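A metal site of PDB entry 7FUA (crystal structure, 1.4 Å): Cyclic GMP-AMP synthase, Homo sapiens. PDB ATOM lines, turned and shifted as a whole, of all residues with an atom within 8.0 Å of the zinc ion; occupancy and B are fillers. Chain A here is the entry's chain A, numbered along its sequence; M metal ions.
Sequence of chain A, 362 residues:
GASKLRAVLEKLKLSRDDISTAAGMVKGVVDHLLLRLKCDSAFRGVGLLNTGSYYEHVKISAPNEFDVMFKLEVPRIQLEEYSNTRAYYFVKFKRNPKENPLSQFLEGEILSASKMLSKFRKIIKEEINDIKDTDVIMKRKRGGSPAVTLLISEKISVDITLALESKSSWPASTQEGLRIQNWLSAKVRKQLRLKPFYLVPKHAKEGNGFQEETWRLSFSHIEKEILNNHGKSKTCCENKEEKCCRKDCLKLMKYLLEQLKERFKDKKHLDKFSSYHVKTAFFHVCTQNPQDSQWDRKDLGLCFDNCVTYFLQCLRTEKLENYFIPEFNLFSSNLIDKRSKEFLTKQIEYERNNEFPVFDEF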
ATOM      1  N   LEU A 227      14.299   6.530  -2.981  1.00  0.00           N
ATOM      2  CA  LEU A 227      13.601   5.660  -2.036  1.00  0.00           C
ATOM      3  C   LEU A 227      12.438   4.925  -2.691  1.00  0.00           C
ATOM      4  O   LEU A 227      12.193   3.747  -2.385  1.00  0.00           O
ATOM      5  CB  LEU A 227      13.103   6.473  -0.846  1.00  0.00           C
ATOM      6  CG  LEU A 227      14.232   6.641   0.151  1.00  0.00           C
ATOM      7  CD1 LEU A 227      13.904   7.751   1.157  1.00  0.00           C
ATOM      8  CD2 LEU A 227      14.450   5.312   0.857  1.00  0.00           C
ATOM      9  N   ASN A 229      12.076   4.163  -5.863  1.00  0.00           N
ATOM     10  CA  ASN A 229      12.501   3.391  -7.026  1.00  0.00           C
ATOM     11  C   ASN A 229      13.925   2.941  -6.686  1.00  0.00           C
ATOM     12  O   ASN A 229      14.912   3.409  -7.253  1.00  0.00           O
ATOM     13  CB  ASN A 229      12.432   4.265  -8.286  1.00  0.00           C
ATOM     14  CG  ASN A 229      12.572   3.465  -9.564  1.00  0.00           C
ATOM     15  OD1 ASN A 229      12.733   2.244  -9.540  1.00  0.00           O
ATOM     16  ND2 ASN A 229      12.523   4.168 -10.692  1.00  0.00           N
ATOM     17  N   HIS A 230      14.021   2.010  -5.720  1.00  0.00           N
ATOM     18  CA  HIS A 230      15.242   1.808  -4.931  1.00  0.00           C
ATOM     19  C   HIS A 230      15.991   0.539  -5.267  1.00  0.00           C
ATOM     20  O   HIS A 230      17.003   0.240  -4.605  1.00  0.00           O
ATOM     21  CB  HIS A 230      14.867   1.728  -3.446  1.00  0.00           C
ATOM     22  CG  HIS A 230      13.881   0.639  -3.157  1.00  0.00           C
ATOM     23  ND1 HIS A 230      12.625   0.896  -2.660  1.00  0.00           N
ATOM     24  CD2 HIS A 230      13.946  -0.708  -3.358  1.00  0.00           C
ATOM     25  CE1 HIS A 230      11.954  -0.242  -2.545  1.00  0.00           C
ATOM     26  NE2 HIS A 230      12.732  -1.228  -2.974  1.00  0.00           N
ATOM     27  N   GLY A 231      15.516  -0.263  -6.221  1.00  0.00           N
ATOM     28  CA  GLY A 231      16.131  -1.542  -6.460  1.00  0.00           C
ATOM     29  C   GLY A 231      17.125  -1.500  -7.600  1.00  0.00           C
ATOM     30  O   GLY A 231      17.066  -0.651  -8.477  1.00  0.00           O
ATOM     31  N   LYS A 232      18.011  -2.479  -7.630  1.00  0.00           N
ATOM     32  CA  LYS A 232      18.717  -2.742  -8.875  1.00  0.00           C
ATOM     33  C   LYS A 232      17.741  -3.199  -9.938  1.00  0.00           C
ATOM     34  O   LYS A 232      17.788  -2.747 -11.089  1.00  0.00           O
ATOM     35  CB  LYS A 232      19.800  -3.793  -8.674  1.00  0.00           C
ATOM     36  CG  LYS A 232      20.538  -4.120  -9.982  1.00  0.00           C
ATOM     37  CD  LYS A 232      21.754  -5.006  -9.792  1.00  0.00           C
ATOM     38  CE  LYS A 232      22.916  -4.243  -9.152  1.00  0.00           C
ATOM     39  NZ  LYS A 232      23.172  -2.927  -9.841  1.00  0.00           N
ATOM     40  N   SER A 233      16.827  -4.103  -9.567  1.00  0.00           N
ATOM     41  CA  SER A 233      15.763  -4.499 -10.483  1.00  0.00           C
ATOM     42  C   SER A 233      14.718  -3.409 -10.586  1.00  0.00           C
ATOM     43  O   SER A 233      14.256  -2.873  -9.565  1.00  0.00           O
ATOM     44  CB  SER A 233      15.086  -5.750  -9.941  1.00  0.00           C
ATOM     45  OG  SER A 233      13.973  -6.059 -10.771  1.00  0.00           O
ATOM     46  N   THR A 235      11.775  -3.914 -11.177  1.00  0.00           N
ATOM     47  CA  THR A 235      10.572  -4.456 -10.544  1.00  0.00           C
ATOM     48  C   THR A 235      10.755  -4.783  -9.076  1.00  0.00           C
ATOM     49  O   THR A 235       9.907  -5.478  -8.497  1.00  0.00           O
ATOM     50  CB  THR A 235      10.015  -5.655 -11.337  1.00  0.00           C
ATOM     51  OG1 THR A 235      11.082  -6.551 -11.664  1.00  0.00           O
ATOM     52  CG2 THR A 235       9.346  -5.184 -12.625  1.00  0.00           C
ATOM     53  N   CYS A 236      11.812  -4.277  -8.437  1.00  0.00           N
ATOM     54  CA  CYS A 236      11.952  -4.474  -6.999  1.00  0.00           C
ATOM     55  C   CYS A 236      10.719  -3.974  -6.282  1.00  0.00           C
ATOM     56  O   CYS A 236      10.204  -2.883  -6.558  1.00  0.00           O
ATOM     57  CB  CYS A 236      13.207  -3.748  -6.463  1.00  0.00           C
ATOM     58  SG  CYS A 236      13.708  -4.184  -4.751  1.00  0.00           S
ATOM     59  N   CYS A 237      10.175  -4.823  -5.415  1.00  0.00           N
ATOM     60  CA  CYS A 237       8.978  -4.529  -4.628  1.00  0.00           C
ATOM     61  C   CYS A 237       7.732  -4.341  -5.479  1.00  0.00           C
ATOM     62  O   CYS A 237       6.740  -3.769  -5.005  1.00  0.00           O
ATOM     63  CB  CYS A 237       9.227  -3.349  -3.678  1.00  0.00           C
ATOM     64  SG  CYS A 237      10.358  -3.770  -2.332  1.00  0.00           S
ATOM     65  N   GLU A 238       7.730  -4.797  -6.738  1.00  0.00           N
ATOM     66  CA  GLU A 238       6.501  -4.855  -7.522  1.00  0.00           C
ATOM     67  C   GLU A 238       5.864  -6.256  -7.564  1.00  0.00           C
ATOM     68  O   GLU A 238       4.807  -6.431  -8.178  1.00  0.00           O
ATOM     69  CB  GLU A 238       6.721  -4.306  -8.952  1.00  0.00           C
ATOM     70  CG  GLU A 238       7.072  -2.798  -9.006  1.00  0.00           C
ATOM     71  CD  GLU A 238       6.915  -2.196 -10.410  1.00  0.00           C
ATOM     72  OE1 GLU A 238       6.711  -2.948 -11.380  1.00  0.00           O
ATOM     73  OE2 GLU A 238       7.001  -0.939 -10.513  1.00  0.00           O
ATOM     74  N   ASN A 239       6.473  -7.226  -6.892  1.00  0.00           N
ATOM     75  CA  ASN A 239       5.966  -8.590  -6.861  1.00  0.00           C
ATOM     76  C   ASN A 239       6.533  -9.306  -5.650  1.00  0.00           C
ATOM     77  O   ASN A 239       7.526  -8.851  -5.053  1.00  0.00           O
ATOM     78  CB  ASN A 239       6.280  -9.358  -8.161  1.00  0.00           C
ATOM     79  CG  ASN A 239       7.767  -9.465  -8.408  1.00  0.00           C
ATOM     80  OD1 ASN A 239       8.457 -10.183  -7.689  1.00  0.00           O
ATOM     81  ND2 ASN A 239       8.283  -8.737  -9.400  1.00  0.00           N
ATOM     82  N   GLU A 242      10.287 -10.291  -5.397  1.00  0.00           N
ATOM     83  CA  GLU A 242      11.267  -9.211  -5.306  1.00  0.00           C
ATOM     84  C   GLU A 242      10.918  -8.238  -4.192  1.00  0.00           C
ATOM     85  O   GLU A 242      11.170  -7.035  -4.306  1.00  0.00           O
ATOM     86  CB  GLU A 242      11.402  -8.483  -6.632  1.00  0.00           C
ATOM     87  CG  GLU A 242      11.825  -9.358  -7.778  1.00  0.00           C
ATOM     88  CD  GLU A 242      12.012  -8.538  -9.024  1.00  0.00           C
ATOM     89  OE1 GLU A 242      13.034  -7.812  -9.078  1.00  0.00           O
ATOM     90  OE2 GLU A 242      11.148  -8.613  -9.925  1.00  0.00           O
ATOM     91  N   LYS A 243      10.383  -8.725  -3.095  1.00  0.00           N
ATOM     92  CA  LYS A 243      10.068  -7.872  -1.945  1.00  0.00           C
ATOM     93  C   LYS A 243      11.342  -7.762  -1.098  1.00  0.00           C
ATOM     94  O   LYS A 243      11.710  -8.691  -0.385  1.00  0.00           O
ATOM     95  CB  LYS A 243       8.909  -8.462  -1.151  1.00  0.00           C
ATOM     96  CG  LYS A 243       8.135  -7.423  -0.361  1.00  0.00           C
ATOM     97  CD  LYS A 243       6.971  -8.038   0.389  1.00  0.00           C
ATOM     98  CE  LYS A 243       6.182  -6.968   1.112  1.00  0.00           C
ATOM     99  NZ  LYS A 243       7.062  -6.125   1.966  1.00  0.00           N
ATOM    100  N   CYS A 244      12.021  -6.617  -1.194  1.00  0.00           N
ATOM    101  CA  CYS A 244      13.239  -6.405  -0.426  1.00  0.00           C
ATOM    102  C   CYS A 244      12.925  -5.732   0.918  1.00  0.00           C
ATOM    103  O   CYS A 244      11.802  -5.292   1.177  1.00  0.00           O
ATOM    104  CB  CYS A 244      14.240  -5.573  -1.237  1.00  0.00           C
ATOM    105  SG  CYS A 244      14.007  -3.772  -1.205  1.00  0.00           S
ATOM    106  N   CYS A 245      13.939  -5.605   1.777  1.00  0.00           N
ATOM    107  CA  CYS A 245      13.754  -5.023   3.092  1.00  0.00           C
ATOM    108  C   CYS A 245      14.413  -3.658   3.249  1.00  0.00           C
ATOM    109  O   CYS A 245      14.630  -3.212   4.378  1.00  0.00           O
ATOM    110  CB  CYS A 245      14.203  -5.987   4.197  1.00  0.00           C
ATOM    111  SG  CYS A 245      15.978  -6.291   4.252  1.00  0.00           S
ATOM    112  N   ARG A 246      14.702  -2.953   2.138  1.00  0.00           N
ATOM    113  CA  ARG A 246      15.379  -1.651   2.246  1.00  0.00           C
ATOM    114  C   ARG A 246      14.558  -0.653   3.051  1.00  0.00           C
ATOM    115  O   ARG A 246      15.050  -0.055   4.029  1.00  0.00           O
ATOM    116  CB  ARG A 246      15.671  -1.082   0.852  1.00  0.00           C
ATOM    117  CG  ARG A 246      16.897  -1.677   0.185  1.00  0.00           C
ATOM    118  CD  ARG A 246      17.110  -1.056  -1.215  1.00  0.00           C
ATOM    119  NE  ARG A 246      18.184  -1.622  -2.003  1.00  0.00           N
ATOM    120  CZ  ARG A 246      18.036  -2.582  -2.928  1.00  0.00           C
ATOM    121  NH1 ARG A 246      19.093  -2.960  -3.647  1.00  0.00           N
ATOM    122  NH2 ARG A 246      16.843  -3.166  -3.110  1.00  0.00           N
ATOM    123  N   LYS A 247      13.288  -0.480   2.687  1.00  0.00           N
ATOM    124  CA  LYS A 247      12.472   0.507   3.376  1.00  0.00           C
ATOM    125  C   LYS A 247      12.254   0.105   4.828  1.00  0.00           C
ATOM    126  O   LYS A 247      12.285   0.959   5.722  1.00  0.00           O
ATOM    127  CB  LYS A 247      11.160   0.742   2.639  1.00  0.00           C
ATOM    128  CG  LYS A 247      11.370   1.513   1.349  1.00  0.00           C
ATOM    129  CD  LYS A 247      10.042   1.982   0.801  1.00  0.00           C
ATOM    130  CE  LYS A 247      10.175   3.374   0.227  1.00  0.00           C
ATOM    131  NZ  LYS A 247       8.989   3.801  -0.527  1.00  0.00           N
ATOM    132  N   ASP A 292      19.948  -6.445  -5.052  1.00  0.00           N
ATOM    133  CA  ASP A 292      18.701  -6.716  -4.337  1.00  0.00           C
ATOM    134  C   ASP A 292      18.803  -7.977  -3.471  1.00  0.00           C
ATOM    135  O   ASP A 292      18.149  -8.068  -2.416  1.00  0.00           O
ATOM    136  CB  ASP A 292      17.528  -6.845  -5.308  1.00  0.00           C
ATOM    137  CG  ASP A 292      17.269  -5.564  -6.101  1.00  0.00           C
ATOM    138  OD1 ASP A 292      17.637  -4.476  -5.615  1.00  0.00           O
ATOM    139  OD2 ASP A 292      16.689  -5.662  -7.205  1.00  0.00           O
ATOM    140  N   TRP A 295      19.377  -7.600   0.173  1.00  0.00           N
ATOM    141  CA  TRP A 295      18.289  -6.996   0.921  1.00  0.00           C
ATOM    142  C   TRP A 295      17.061  -7.895   0.909  1.00  0.00           C
ATOM    143  O   TRP A 295      15.916  -7.419   0.907  1.00  0.00           O
ATOM    144  CB  TRP A 295      17.940  -5.610   0.350  1.00  0.00           C
ATOM    145  CG  TRP A 295      19.050  -4.644   0.442  1.00  0.00           C
ATOM    146  CD1 TRP A 295      20.018  -4.412  -0.504  1.00  0.00           C
ATOM    147  CD2 TRP A 295      19.352  -3.782   1.546  1.00  0.00           C
ATOM    148  NE1 TRP A 295      20.882  -3.422  -0.056  1.00  0.00           N
ATOM    149  CE2 TRP A 295      20.497  -3.033   1.199  1.00  0.00           C
ATOM    150  CE3 TRP A 295      18.744  -3.568   2.787  1.00  0.00           C
ATOM    151  CZ2 TRP A 295      21.048  -2.077   2.052  1.00  0.00           C
ATOM    152  CZ3 TRP A 295      19.286  -2.638   3.633  1.00  0.00           C
ATOM    153  CH2 TRP A 295      20.425  -1.896   3.267  1.00  0.00           C
HETATM  154 ZN    ZN M   1      12.519  -3.283  -3.040  1.00  0.00          ZN
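The backbone carbonyl oxygen (O) of His 230 lies within hydrogen-bond range of the guanidinium group (NE) of Arg 246, 3.4 Å away.
The backbone carbonyl oxygen (O) of Leu 227 lies within hydrogen-bond range of a ring nitrogen (ND1) of His 230 (2.9 Å).
The guanidinium group of Arg 246 sits close to the side-chain sulfur of Cys 236 (3.7 Å).
The backbone carbonyl oxygen (O) of Glu 242 is in hydrogen-bond range of the backbone NH (N) of Cys 237 (2.7 Å).
SG of Cys 244 lies close to NH2 of Arg 246, 3.5 Å away.
Four residues have an atom within 4 Å of the zinc ion: His 230, Cys 236, Cys 237 and Cys 244.
Along chain A the residues within 4 Å of the zinc ion span positions 230 to 244.
The nearest printed residue that does not touch the zinc ion is Glu 242 (4.2 Å).
The zinc ion is bound by a ring nitrogen (NE2) of His 230.
SG of Cys 236 binds the zinc ion (2.3 Å).
The zinc ion is bound by SG of Cys 237.
The zinc ion is bound by SG of Cys 244 (2.4 Å).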
